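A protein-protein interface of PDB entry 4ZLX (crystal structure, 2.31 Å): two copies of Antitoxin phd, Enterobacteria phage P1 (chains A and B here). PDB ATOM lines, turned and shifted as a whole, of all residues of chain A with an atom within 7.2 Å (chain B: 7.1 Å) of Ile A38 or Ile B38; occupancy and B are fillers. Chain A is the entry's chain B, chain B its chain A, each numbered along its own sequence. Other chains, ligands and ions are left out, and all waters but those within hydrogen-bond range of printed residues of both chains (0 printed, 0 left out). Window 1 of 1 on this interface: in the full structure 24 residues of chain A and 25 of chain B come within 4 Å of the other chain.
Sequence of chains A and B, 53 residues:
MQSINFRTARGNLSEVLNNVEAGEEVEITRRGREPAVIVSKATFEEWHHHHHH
Ile B28 touches Leu A17 (CG2 to CD1, 3.9 Å). Ala B36 touches Leu A17 (CB to CD2, 3.7 Å). CZ of Phe B44 touches OE1 of Glu A25 (3.3 Å). Ala A36 touches Val B39. Val B37 touches Val A37 (O to O, 3.7 Å). Ile A38 touches Ala B36 (CG2 to CB, 3.8 Å). Ile A38 touches Ile B38. Met B1 touches Phe A44 (CE to CE2, 3.6 Å). Phe A44 touches Glu B25. Trp A47 touches Phe B44 (CZ2 to CD1, 3.7 Å).
The backbone NH (N) of Val B37 sits at hydrogen-bond distance from the backbone carbonyl oxygen (O) of Val A39 (2.7 Å). O of Val B39 lies within hydrogen-bond range of N of Val A37, 2.8 Å away.
Glu A25 touches Phe B44, and with the chains exchanged Phe A44 touches Glu B25. Val B37 touches its own counterpart, Val A37. Val A37 touches Val B39, and with the chains exchanged Val A39 touches Val B37. Val A37 touches Phe B44, and with the chains exchanged Phe A44 touches Val B37. Of the 22 pairs that touch across the chains among the printed residues, 20 have their exchanged pair printed and touching as well.
Ala A9 touches none of the printed residues of chain B. Printed residues of chain B within 4 Å of Glu A25: Phe B44 (3.3 Å). Of the printed residues of chain B, Ile A28 touches Leu B17. Ile A38 touches three residues of chain B. Of the printed residues of chain A, Glu B25 touches Phe A44. Of the printed residues of chain A, Ala B36 touches Leu A17 (3.7 Å), Ile A38 (3.8 Å) and Val A39 (3.5 Å). Ile B38 touches just these residues of chain A: Ala A36, Val A37 and Ile A38. Thr B43 touches none of the printed residues of chain A. Of the printed residues of chain A, Phe B44 touches Met A1 (3.9 Å), Glu A25 (3.3 Å), Val A37 (3.8 Å) and Trp A47 (3.7 Å). The nearest residue of chain B that does not touch Ile A38 is Val B39 (5.2 Å). The nearest printed residue of chain B that does not touch Met A1 is Ser B40 (8.5 Å).
O of Val B26 lies within hydrogen-bond range of N of Ile B38. N of Ile B28 lies within hydrogen-bond range of O of Ala B36 (2.6 Å). O of Val A26 lies within hydrogen-bond range of N of Ile A38 (2.8 Å). N of Ile A28 is in hydrogen-bond range of O of Ala A36, at 2.8 Å.
Of the 19 printed residues of chain A, 11 touch a printed residue of chain B. Hydrophobic or aromatic side chains of chain A within 4 Å of the printed part of chain B: Met A1, Leu A13, Leu A17, Ile A28, Ala A36, Val A37, Ile A38, Val A39, Phe A44 and Trp A47. Of the 19 printed residues of chain B, 10 touch a printed residue of chain A. Among the printed residues, no Asp or Glu carboxylate lies within 4 Å of a Lys or Arg side-chain nitrogen of the other chain.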
ATOM      1  N   MET A   1       8.024  12.698  30.840  1.00  0.00           N
ATOM      2  CA  MET A   1       7.023  12.961  29.807  1.00  0.00           C
ATOM      3  C   MET A   1       7.475  12.459  28.441  1.00  0.00           C
ATOM      4  O   MET A   1       8.514  12.877  27.924  1.00  0.00           O
ATOM      5  CB  MET A   1       6.641  14.452  29.759  1.00  0.00           C
ATOM      6  CG  MET A   1       5.541  14.768  28.763  1.00  0.00           C
ATOM      7  SD  MET A   1       4.938  16.459  28.887  1.00  0.00           S
ATOM      8  CE  MET A   1       6.213  17.333  27.985  1.00  0.00           C
ATOM      9  N   ILE A   4       5.270  11.910  21.118  1.00  0.00           N
ATOM     10  CA  ILE A   4       4.953  11.231  19.866  1.00  0.00           C
ATOM     11  C   ILE A   4       4.363  12.245  18.877  1.00  0.00           C
ATOM     12  O   ILE A   4       3.704  13.201  19.286  1.00  0.00           O
ATOM     13  CB  ILE A   4       3.953  10.082  20.079  1.00  0.00           C
ATOM     14  CG1 ILE A   4       2.647  10.616  20.671  1.00  0.00           C
ATOM     15  CG2 ILE A   4       4.553   9.013  20.980  1.00  0.00           C
ATOM     16  CD1 ILE A   4       1.490   9.646  20.571  1.00  0.00           C
ATOM     17  N   ALA A   9       0.331   9.048  16.896  1.00  0.00           N
ATOM     18  CA  ALA A   9      -0.740   9.109  17.899  1.00  0.00           C
ATOM     19  C   ALA A   9      -2.101   8.728  17.330  1.00  0.00           C
ATOM     20  O   ALA A   9      -2.812   7.932  17.950  1.00  0.00           O
ATOM     21  CB  ALA A   9      -0.823  10.499  18.501  1.00  0.00           C
ATOM     22  N   LEU A  13      -3.828   5.524  18.975  1.00  0.00           N
ATOM     23  CA  LEU A  13      -4.413   6.210  20.131  1.00  0.00           C
ATOM     24  C   LEU A  13      -4.736   5.333  21.320  1.00  0.00           C
ATOM     25  O   LEU A  13      -4.594   5.770  22.450  1.00  0.00           O
ATOM     26  CB  LEU A  13      -5.592   7.108  19.752  1.00  0.00           C
ATOM     27  CG  LEU A  13      -5.975   8.175  20.779  1.00  0.00           C
ATOM     28  CD1 LEU A  13      -4.826   9.198  21.000  1.00  0.00           C
ATOM     29  CD2 LEU A  13      -7.279   8.813  20.395  1.00  0.00           C
ATOM     30  N   VAL A  16      -1.581   4.722  23.247  1.00  0.00           N
ATOM     31  CA  VAL A  16      -1.279   6.017  23.862  1.00  0.00           C
ATOM     32  C   VAL A  16      -2.136   6.164  25.115  1.00  0.00           C
ATOM     33  O   VAL A  16      -1.613   6.523  26.168  1.00  0.00           O
ATOM     34  CB  VAL A  16      -1.514   7.179  22.849  1.00  0.00           C
ATOM     35  CG1 VAL A  16      -1.564   8.549  23.530  1.00  0.00           C
ATOM     36  CG2 VAL A  16      -0.467   7.164  21.736  1.00  0.00           C
ATOM     37  N   LEU A  17      -3.436   5.847  25.019  1.00  0.00           N
ATOM     38  CA  LEU A  17      -4.322   6.009  26.163  1.00  0.00           C
ATOM     39  C   LEU A  17      -4.074   4.998  27.271  1.00  0.00           C
ATOM     40  O   LEU A  17      -4.213   5.352  28.432  1.00  0.00           O
ATOM     41  CB  LEU A  17      -5.802   6.129  25.771  1.00  0.00           C
ATOM     42  CG  LEU A  17      -6.161   7.247  24.758  1.00  0.00           C
ATOM     43  CD1 LEU A  17      -7.632   7.251  24.473  1.00  0.00           C
ATOM     44  CD2 LEU A  17      -5.656   8.645  25.195  1.00  0.00           C
ATOM     45  N   VAL A  20      -0.973   6.311  29.011  1.00  0.00           N
ATOM     46  CA  VAL A  20      -1.421   7.443  29.832  1.00  0.00           C
ATOM     47  C   VAL A  20      -2.042   6.935  31.155  1.00  0.00           C
ATOM     48  O   VAL A  20      -1.690   7.429  32.227  1.00  0.00           O
ATOM     49  CB  VAL A  20      -2.340   8.429  29.037  1.00  0.00           C
ATOM     50  CG1 VAL A  20      -3.089   9.390  29.952  1.00  0.00           C
ATOM     51  CG2 VAL A  20      -1.534   9.214  28.006  1.00  0.00           C
ATOM     52  N   GLU A  24       1.967   7.444  32.411  1.00  0.00           N
ATOM     53  CA  GLU A  24       2.727   8.325  31.538  1.00  0.00           C
ATOM     54  C   GLU A  24       1.946   9.583  31.179  1.00  0.00           C
ATOM     55  O   GLU A  24       0.728   9.552  31.076  1.00  0.00           O
ATOM     56  CB  GLU A  24       3.064   7.588  30.236  1.00  0.00           C
ATOM     57  CG  GLU A  24       4.324   6.739  30.259  1.00  0.00           C
ATOM     58  CD  GLU A  24       4.459   5.818  29.057  1.00  0.00           C
ATOM     59  OE1 GLU A  24       4.125   6.249  27.928  1.00  0.00           O
ATOM     60  OE2 GLU A  24       4.881   4.654  29.247  1.00  0.00           O
ATOM     61  N   GLU A  25       2.652  10.681  30.970  1.00  0.00           N
ATOM     62  CA  GLU A  25       2.065  11.926  30.456  1.00  0.00           C
ATOM     63  C   GLU A  25       2.672  11.985  29.056  1.00  0.00           C
ATOM     64  O   GLU A  25       3.884  11.857  28.905  1.00  0.00           O
ATOM     65  CB  GLU A  25       2.438  13.147  31.300  1.00  0.00           C
ATOM     66  CG  GLU A  25       1.777  13.173  32.661  1.00  0.00           C
ATOM     67  CD  GLU A  25       2.291  14.247  33.595  1.00  0.00           C
ATOM     68  OE1 GLU A  25       3.312  14.895  33.270  1.00  0.00           O
ATOM     69  OE2 GLU A  25       1.699  14.403  34.686  1.00  0.00           O
ATOM     70  N   VAL A  26       1.827  12.014  28.040  1.00  0.00           N
ATOM     71  CA  VAL A  26       2.259  11.942  26.651  1.00  0.00           C
ATOM     72  C   VAL A  26       2.025  13.261  25.933  1.00  0.00           C
ATOM     73  O   VAL A  26       0.937  13.813  25.972  1.00  0.00           O
ATOM     74  CB  VAL A  26       1.549  10.766  25.928  1.00  0.00           C
ATOM     75  CG1 VAL A  26       2.021  10.641  24.487  1.00  0.00           C
ATOM     76  CG2 VAL A  26       1.719   9.437  26.686  1.00  0.00           C
ATOM     77  N   GLU A  27       3.051  13.739  25.243  1.00  0.00           N
ATOM     78  CA  GLU A  27       2.983  14.947  24.448  1.00  0.00           C
ATOM     79  C   GLU A  27       2.794  14.592  22.981  1.00  0.00           C
ATOM     80  O   GLU A  27       3.610  13.862  22.424  1.00  0.00           O
ATOM     81  CB  GLU A  27       4.271  15.746  24.654  1.00  0.00           C
ATOM     82  CG  GLU A  27       4.301  17.029  23.875  1.00  0.00           C
ATOM     83  CD  GLU A  27       5.444  17.923  24.290  1.00  0.00           C
ATOM     84  OE1 GLU A  27       5.188  18.872  25.059  1.00  0.00           O
ATOM     85  OE2 GLU A  27       6.598  17.655  23.887  1.00  0.00           O
ATOM     86  N   ILE A  28       1.723  15.105  22.360  1.00  0.00           N
ATOM     87  CA  ILE A  28       1.466  14.920  20.931  1.00  0.00           C
ATOM     88  C   ILE A  28       1.997  16.134  20.189  1.00  0.00           C
ATOM     89  O   ILE A  28       1.569  17.260  20.465  1.00  0.00           O
ATOM     90  CB  ILE A  28      -0.010  14.616  20.553  1.00  0.00           C
ATOM     91  CG1 ILE A  28      -0.571  13.412  21.342  1.00  0.00           C
ATOM     92  CG2 ILE A  28      -0.153  14.417  19.023  1.00  0.00           C
ATOM     93  CD1 ILE A  28      -2.024  13.210  21.063  1.00  0.00           C
ATOM     94  N   ALA A  36       0.213  19.179  22.378  1.00  0.00           N
ATOM     95  CA  ALA A  36      -0.890  18.889  23.302  1.00  0.00           C
ATOM     96  C   ALA A  36      -0.391  17.843  24.282  1.00  0.00           C
ATOM     97  O   ALA A  36       0.401  16.974  23.909  1.00  0.00           O
ATOM     98  CB  ALA A  36      -2.088  18.355  22.543  1.00  0.00           C
ATOM     99  N   VAL A  37      -0.820  17.923  25.540  1.00  0.00           N
ATOM    100  CA  VAL A  37      -0.382  16.938  26.530  1.00  0.00           C
ATOM    101  C   VAL A  37      -1.596  16.122  26.984  1.00  0.00           C
ATOM    102  O   VAL A  37      -2.637  16.696  27.334  1.00  0.00           O
ATOM    103  CB  VAL A  37       0.400  17.565  27.729  1.00  0.00           C
ATOM    104  CG1 VAL A  37       0.961  16.478  28.666  1.00  0.00           C
ATOM    105  CG2 VAL A  37       1.515  18.498  27.237  1.00  0.00           C
ATOM    106  N   ILE A  38      -1.452  14.792  26.979  1.00  0.00           N
ATOM    107  CA  ILE A  38      -2.509  13.893  27.428  1.00  0.00           C
ATOM    108  C   ILE A  38      -2.135  13.345  28.789  1.00  0.00           C
ATOM    109  O   ILE A  38      -1.093  12.698  28.935  1.00  0.00           O
ATOM    110  CB  ILE A  38      -2.846  12.737  26.432  1.00  0.00           C
ATOM    111  CG1 ILE A  38      -2.998  13.248  24.984  1.00  0.00           C
ATOM    112  CG2 ILE A  38      -4.101  11.957  26.924  1.00  0.00           C
ATOM    113  CD1 ILE A  38      -3.099  12.193  24.023  1.00  0.00           C
ATOM    114  N   VAL A  39      -3.012  13.591  29.770  1.00  0.00           N
ATOM    115  CA  VAL A  39      -2.878  13.120  31.145  1.00  0.00           C
ATOM    116  C   VAL A  39      -4.074  12.265  31.520  1.00  0.00           C
ATOM    117  O   VAL A  39      -5.106  12.310  30.859  1.00  0.00           O
ATOM    118  CB  VAL A  39      -2.637  14.260  32.181  1.00  0.00           C
ATOM    119  CG1 VAL A  39      -1.371  15.047  31.844  1.00  0.00           C
ATOM    120  CG2 VAL A  39      -3.862  15.181  32.303  1.00  0.00           C
ATOM    121  N   SER A  40      -3.926  11.474  32.580  1.00  0.00           N
ATOM    122  CA  SER A  40      -5.001  10.658  33.083  1.00  0.00           C
ATOM    123  C   SER A  40      -5.950  11.600  33.801  1.00  0.00           C
ATOM    124  O   SER A  40      -5.526  12.652  34.291  1.00  0.00           O
ATOM    125  CB  SER A  40      -4.463   9.608  34.058  1.00  0.00           C
ATOM    126  OG  SER A  40      -3.818  10.207  35.173  1.00  0.00           O
ATOM    127  N   PHE A  44      -5.176  14.919  36.135  1.00  0.00           N
ATOM    128  CA  PHE A  44      -5.928  16.147  35.916  1.00  0.00           C
ATOM    129  C   PHE A  44      -6.686  16.610  37.187  1.00  0.00           C
ATOM    130  O   PHE A  44      -6.710  17.804  37.487  1.00  0.00           O
ATOM    131  CB  PHE A  44      -6.894  15.969  34.747  1.00  0.00           C
ATOM    132  CG  PHE A  44      -7.732  17.190  34.485  1.00  0.00           C
ATOM    133  CD1 PHE A  44      -7.194  18.298  33.839  1.00  0.00           C
ATOM    134  CD2 PHE A  44      -9.054  17.245  34.903  1.00  0.00           C
ATOM    135  CE1 PHE A  44      -7.966  19.436  33.613  1.00  0.00           C
ATOM    136  CE2 PHE A  44      -9.828  18.385  34.665  1.00  0.00           C
ATOM    137  CZ  PHE A  44      -9.278  19.470  34.023  1.00  0.00           C
ATOM    138  N   TRP A  47      -4.530  18.325  39.974  1.00  0.00           N
ATOM    139  CA  TRP A  47      -4.106  19.717  39.742  1.00  0.00           C
ATOM    140  C   TRP A  47      -4.946  20.730  40.542  1.00  0.00           C
ATOM    141  O   TRP A  47      -6.106  20.996  40.218  1.00  0.00           O
ATOM    142  CB  TRP A  47      -4.117  20.067  38.242  1.00  0.00           C
ATOM    143  CG  TRP A  47      -3.045  19.414  37.422  1.00  0.00           C
ATOM    144  CD1 TRP A  47      -1.868  18.886  37.868  1.00  0.00           C
ATOM    145  CD2 TRP A  47      -3.041  19.257  35.993  1.00  0.00           C
ATOM    146  NE1 TRP A  47      -1.137  18.394  36.808  1.00  0.00           N
ATOM    147  CE2 TRP A  47      -1.823  18.631  35.644  1.00  0.00           C
ATOM    148  CE3 TRP A  47      -3.956  19.575  34.970  1.00  0.00           C
ATOM    149  CZ2 TRP A  47      -1.489  18.338  34.317  1.00  0.00           C
ATOM    150  CZ3 TRP A  47      -3.612  19.300  33.656  1.00  0.00           C
ATOM    151  CH2 TRP A  47      -2.405  18.667  33.344  1.00  0.00           C
ATOM    152  N   MET B   1     -14.633  22.162  30.004  1.00  0.00           N
ATOM    153  CA  MET B   1     -14.399  20.725  29.941  1.00  0.00           C
ATOM    154  C   MET B   1     -15.402  19.962  29.049  1.00  0.00           C
ATOM    155  O   MET B   1     -16.491  19.582  29.485  1.00  0.00           O
ATOM    156  CB  MET B   1     -14.290  20.111  31.349  1.00  0.00           C
ATOM    157  CG  MET B   1     -13.931  18.628  31.356  1.00  0.00           C
ATOM    158  SD  MET B   1     -12.181  18.266  31.083  1.00  0.00           S
ATOM    159  CE  MET B   1     -11.990  16.953  32.211  1.00  0.00           C
ATOM    160  N   ILE B   4     -15.608  13.592  24.877  1.00  0.00           N
ATOM    161  CA  ILE B   4     -15.810  12.840  23.632  1.00  0.00           C
ATOM    162  C   ILE B   4     -15.429  11.382  23.852  1.00  0.00           C
ATOM    163  O   ILE B   4     -14.692  11.089  24.791  1.00  0.00           O
ATOM    164  CB  ILE B   4     -15.121  13.459  22.375  1.00  0.00           C
ATOM    165  CG1 ILE B   4     -13.591  13.583  22.561  1.00  0.00           C
ATOM    166  CG2 ILE B   4     -15.806  14.781  21.929  1.00  0.00           C
ATOM    167  CD1 ILE B   4     -12.835  14.095  21.421  1.00  0.00           C
ATOM    168  N   ALA B   9     -12.468  10.836  19.230  1.00  0.00           N
ATOM    169  CA  ALA B   9     -11.087  11.320  19.385  1.00  0.00           C
ATOM    170  C   ALA B   9     -10.205  10.805  18.224  1.00  0.00           C
ATOM    171  O   ALA B   9      -9.544  11.603  17.569  1.00  0.00           O
ATOM    172  CB  ALA B   9     -10.504  10.858  20.719  1.00  0.00           C
ATOM    173  N   LEU B  13      -9.019  13.571  15.501  1.00  0.00           N
ATOM    174  CA  LEU B  13      -7.871  14.076  16.275  1.00  0.00           C
ATOM    175  C   LEU B  13      -7.341  15.465  15.923  1.00  0.00           C
ATOM    176  O   LEU B  13      -7.084  16.257  16.825  1.00  0.00           O
ATOM    177  CB  LEU B  13      -6.739  13.048  16.355  1.00  0.00           C
ATOM    178  CG  LEU B  13      -5.773  13.226  17.522  1.00  0.00           C
ATOM    179  CD1 LEU B  13      -6.531  13.261  18.890  1.00  0.00           C
ATOM    180  CD2 LEU B  13      -4.650  12.172  17.471  1.00  0.00           C
ATOM    181  N   VAL B  16      -9.796  17.968  17.201  1.00  0.00           N
ATOM    182  CA  VAL B  16      -9.739  17.867  18.656  1.00  0.00           C
ATOM    183  C   VAL B  16      -8.533  18.679  19.175  1.00  0.00           C
ATOM    184  O   VAL B  16      -8.702  19.532  20.047  1.00  0.00           O
ATOM    185  CB  VAL B  16      -9.738  16.379  19.125  1.00  0.00           C
ATOM    186  CG1 VAL B  16      -9.378  16.242  20.601  1.00  0.00           C
ATOM    187  CG2 VAL B  16     -11.088  15.737  18.843  1.00  0.00           C
ATOM    188  N   LEU B  17      -7.352  18.469  18.578  1.00  0.00           N
ATOM    189  CA  LEU B  17      -6.127  19.185  18.935  1.00  0.00           C
ATOM    190  C   LEU B  17      -6.196  20.675  18.604  1.00  0.00           C
ATOM    191  O   LEU B  17      -5.490  21.471  19.231  1.00  0.00           O
ATOM    192  CB  LEU B  17      -4.889  18.522  18.285  1.00  0.00           C
ATOM    193  CG  LEU B  17      -4.559  17.062  18.691  1.00  0.00           C
ATOM    194  CD1 LEU B  17      -3.203  16.612  18.072  1.00  0.00           C
ATOM    195  CD2 LEU B  17      -4.518  16.881  20.191  1.00  0.00           C
ATOM    196  N   VAL B  20      -8.152  22.135  21.602  1.00  0.00           N
ATOM    197  CA  VAL B  20      -7.216  22.151  22.724  1.00  0.00           C
ATOM    198  C   VAL B  20      -6.243  23.350  22.650  1.00  0.00           C
ATOM    199  O   VAL B  20      -6.049  24.054  23.643  1.00  0.00           O
ATOM    200  CB  VAL B  20      -6.511  20.776  22.819  1.00  0.00           C
ATOM    201  CG1 VAL B  20      -5.203  20.837  23.597  1.00  0.00           C
ATOM    202  CG2 VAL B  20      -7.446  19.739  23.416  1.00  0.00           C
ATOM    203  N   GLU B  24      -9.492  25.023  25.103  1.00  0.00           N
ATOM    204  CA  GLU B  24     -10.394  23.944  25.521  1.00  0.00           C
ATOM    205  C   GLU B  24      -9.643  22.724  26.126  1.00  0.00           C
ATOM    206  O   GLU B  24      -8.521  22.420  25.719  1.00  0.00           O
ATOM    207  CB  GLU B  24     -11.273  23.528  24.319  1.00  0.00           C
ATOM    208  CG  GLU B  24     -12.399  22.552  24.619  1.00  0.00           C
ATOM    209  CD  GLU B  24     -13.287  22.233  23.432  1.00  0.00           C
ATOM    210  OE1 GLU B  24     -14.044  23.130  22.993  1.00  0.00           O
ATOM    211  OE2 GLU B  24     -13.259  21.070  22.969  1.00  0.00           O
ATOM    212  N   GLU B  25     -10.265  22.070  27.129  1.00  0.00           N
ATOM    213  CA  GLU B  25      -9.776  20.847  27.810  1.00  0.00           C
ATOM    214  C   GLU B  25     -10.758  19.736  27.457  1.00  0.00           C
ATOM    215  O   GLU B  25     -11.968  19.855  27.699  1.00  0.00           O
ATOM    216  CB  GLU B  25      -9.656  21.032  29.324  1.00  0.00           C
ATOM    217  CG  GLU B  25      -8.653  22.111  29.706  1.00  0.00           C
ATOM    218  CD  GLU B  25      -8.525  22.396  31.191  1.00  0.00           C
ATOM    219  OE1 GLU B  25      -9.559  22.674  31.837  1.00  0.00           O
ATOM    220  OE2 GLU B  25      -7.384  22.377  31.701  1.00  0.00           O
ATOM    221  N   VAL B  26     -10.245  18.704  26.796  1.00  0.00           N
ATOM    222  CA  VAL B  26     -11.047  17.620  26.250  1.00  0.00           C
ATOM    223  C   VAL B  26     -10.772  16.308  26.969  1.00  0.00           C
ATOM    224  O   VAL B  26      -9.663  15.775  26.922  1.00  0.00           O
ATOM    225  CB  VAL B  26     -10.819  17.479  24.712  1.00  0.00           C
ATOM    226  CG1 VAL B  26     -11.734  16.427  24.110  1.00  0.00           C
ATOM    227  CG2 VAL B  26     -10.986  18.814  23.991  1.00  0.00           C
ATOM    228  N   GLU B  27     -11.816  15.752  27.544  1.00  0.00           N
ATOM    229  CA  GLU B  27     -11.762  14.456  28.182  1.00  0.00           C
ATOM    230  C   GLU B  27     -12.140  13.373  27.139  1.00  0.00           C
ATOM    231  O   GLU B  27     -13.092  13.555  26.370  1.00  0.00           O
ATOM    232  CB  GLU B  27     -12.719  14.476  29.364  1.00  0.00           C
ATOM    233  CG  GLU B  27     -12.778  13.190  30.145  1.00  0.00           C
ATOM    234  CD  GLU B  27     -13.768  13.248  31.282  1.00  0.00           C
ATOM    235  OE1 GLU B  27     -14.894  12.737  31.117  1.00  0.00           O
ATOM    236  OE2 GLU B  27     -13.457  13.904  32.295  1.00  0.00           O
ATOM    237  N   ILE B  28     -11.353  12.286  27.073  1.00  0.00           N
ATOM    238  CA  ILE B  28     -11.588  11.182  26.147  1.00  0.00           C
ATOM    239  C   ILE B  28     -12.060   9.977  26.934  1.00  0.00           C
ATOM    240  O   ILE B  28     -11.277   9.370  27.674  1.00  0.00           O
ATOM    241  CB  ILE B  28     -10.372  10.830  25.225  1.00  0.00           C
ATOM    242  CG1 ILE B  28      -9.873  12.032  24.415  1.00  0.00           C
ATOM    243  CG2 ILE B  28     -10.719   9.638  24.302  1.00  0.00           C
ATOM    244  CD1 ILE B  28      -8.565  11.715  23.715  1.00  0.00           C
ATOM    245  N   ALA B  36      -9.146   9.937  29.705  1.00  0.00           N
ATOM    246  CA  ALA B  36      -7.894  10.672  29.480  1.00  0.00           C
ATOM    247  C   ALA B  36      -8.285  12.129  29.289  1.00  0.00           C
ATOM    248  O   ALA B  36      -9.404  12.405  28.861  1.00  0.00           O
ATOM    249  CB  ALA B  36      -7.195  10.156  28.235  1.00  0.00           C
ATOM    250  N   VAL B  37      -7.423  13.071  29.701  1.00  0.00           N
ATOM    251  CA  VAL B  37      -7.711  14.498  29.503  1.00  0.00           C
ATOM    252  C   VAL B  37      -6.587  15.087  28.643  1.00  0.00           C
ATOM    253  O   VAL B  37      -5.417  14.854  28.945  1.00  0.00           O
ATOM    254  CB  VAL B  37      -7.922  15.301  30.820  1.00  0.00           C
ATOM    255  CG1 VAL B  37      -8.295  16.752  30.517  1.00  0.00           C
ATOM    256  CG2 VAL B  37      -8.992  14.650  31.732  1.00  0.00           C
ATOM    257  N   ILE B  38      -6.952  15.778  27.540  1.00  0.00           N
ATOM    258  CA  ILE B  38      -6.045  16.469  26.630  1.00  0.00           C
ATOM    259  C   ILE B  38      -6.166  17.939  26.968  1.00  0.00           C
ATOM    260  O   ILE B  38      -7.279  18.496  27.014  1.00  0.00           O
ATOM    261  CB  ILE B  38      -6.291  16.243  25.120  1.00  0.00           C
ATOM    262  CG1 ILE B  38      -6.592  14.760  24.797  1.00  0.00           C
ATOM    263  CG2 ILE B  38      -5.079  16.795  24.308  1.00  0.00           C
ATOM    264  CD1 ILE B  38      -6.496  14.384  23.270  1.00  0.00           C
ATOM    265  N   VAL B  39      -5.001  18.545  27.193  1.00  0.00           N
ATOM    266  CA  VAL B  39      -4.844  19.958  27.517  1.00  0.00           C
ATOM    267  C   VAL B  39      -3.653  20.504  26.726  1.00  0.00           C
ATOM    268  O   VAL B  39      -2.768  19.747  26.329  1.00  0.00           O
ATOM    269  CB  VAL B  39      -4.603  20.174  29.020  1.00  0.00           C
ATOM    270  CG1 VAL B  39      -5.800  19.690  29.825  1.00  0.00           C
ATOM    271  CG2 VAL B  39      -3.333  19.464  29.462  1.00  0.00           C
ATOM    272  N   SER B  40      -3.634  21.814  26.495  1.00  0.00           N
ATOM    273  CA  SER B  40      -2.559  22.461  25.731  1.00  0.00           C
ATOM    274  C   SER B  40      -1.243  22.379  26.520  1.00  0.00           C
ATOM    275  O   SER B  40      -1.286  22.137  27.726  1.00  0.00           O
ATOM    276  CB  SER B  40      -2.919  23.923  25.451  1.00  0.00           C
ATOM    277  OG  SER B  40      -2.989  24.679  26.645  1.00  0.00           O
ATOM    278  N   THR B  43      -1.316  25.080  29.220  1.00  0.00           N
ATOM    279  CA  THR B  43      -2.147  24.708  30.372  1.00  0.00           C
ATOM    280  C   THR B  43      -1.344  23.721  31.222  1.00  0.00           C
ATOM    281  O   THR B  43      -1.316  23.814  32.455  1.00  0.00           O
ATOM    282  CB  THR B  43      -3.462  24.080  29.894  1.00  0.00           C
ATOM    283  OG1 THR B  43      -4.274  25.081  29.306  1.00  0.00           O
ATOM    284  CG2 THR B  43      -4.226  23.374  31.006  1.00  0.00           C
ATOM    285  N   PHE B  44      -0.692  22.782  30.548  1.00  0.00           N
ATOM    286  CA  PHE B  44       0.131  21.799  31.219  1.00  0.00           C
ATOM    287  C   PHE B  44       1.202  22.478  32.084  1.00  0.00           C
ATOM    288  O   PHE B  44       1.318  22.150  33.258  1.00  0.00           O
ATOM    289  CB  PHE B  44       0.755  20.801  30.218  1.00  0.00           C
ATOM    290  CG  PHE B  44       1.635  19.809  30.941  1.00  0.00           C
ATOM    291  CD1 PHE B  44       1.078  18.791  31.710  1.00  0.00           C
ATOM    292  CD2 PHE B  44       3.021  19.936  30.916  1.00  0.00           C
ATOM    293  CE1 PHE B  44       1.892  17.897  32.413  1.00  0.00           C
ATOM    294  CE2 PHE B  44       3.834  19.049  31.634  1.00  0.00           C
ATOM    295  CZ  PHE B  44       3.265  18.033  32.370  1.00  0.00           C
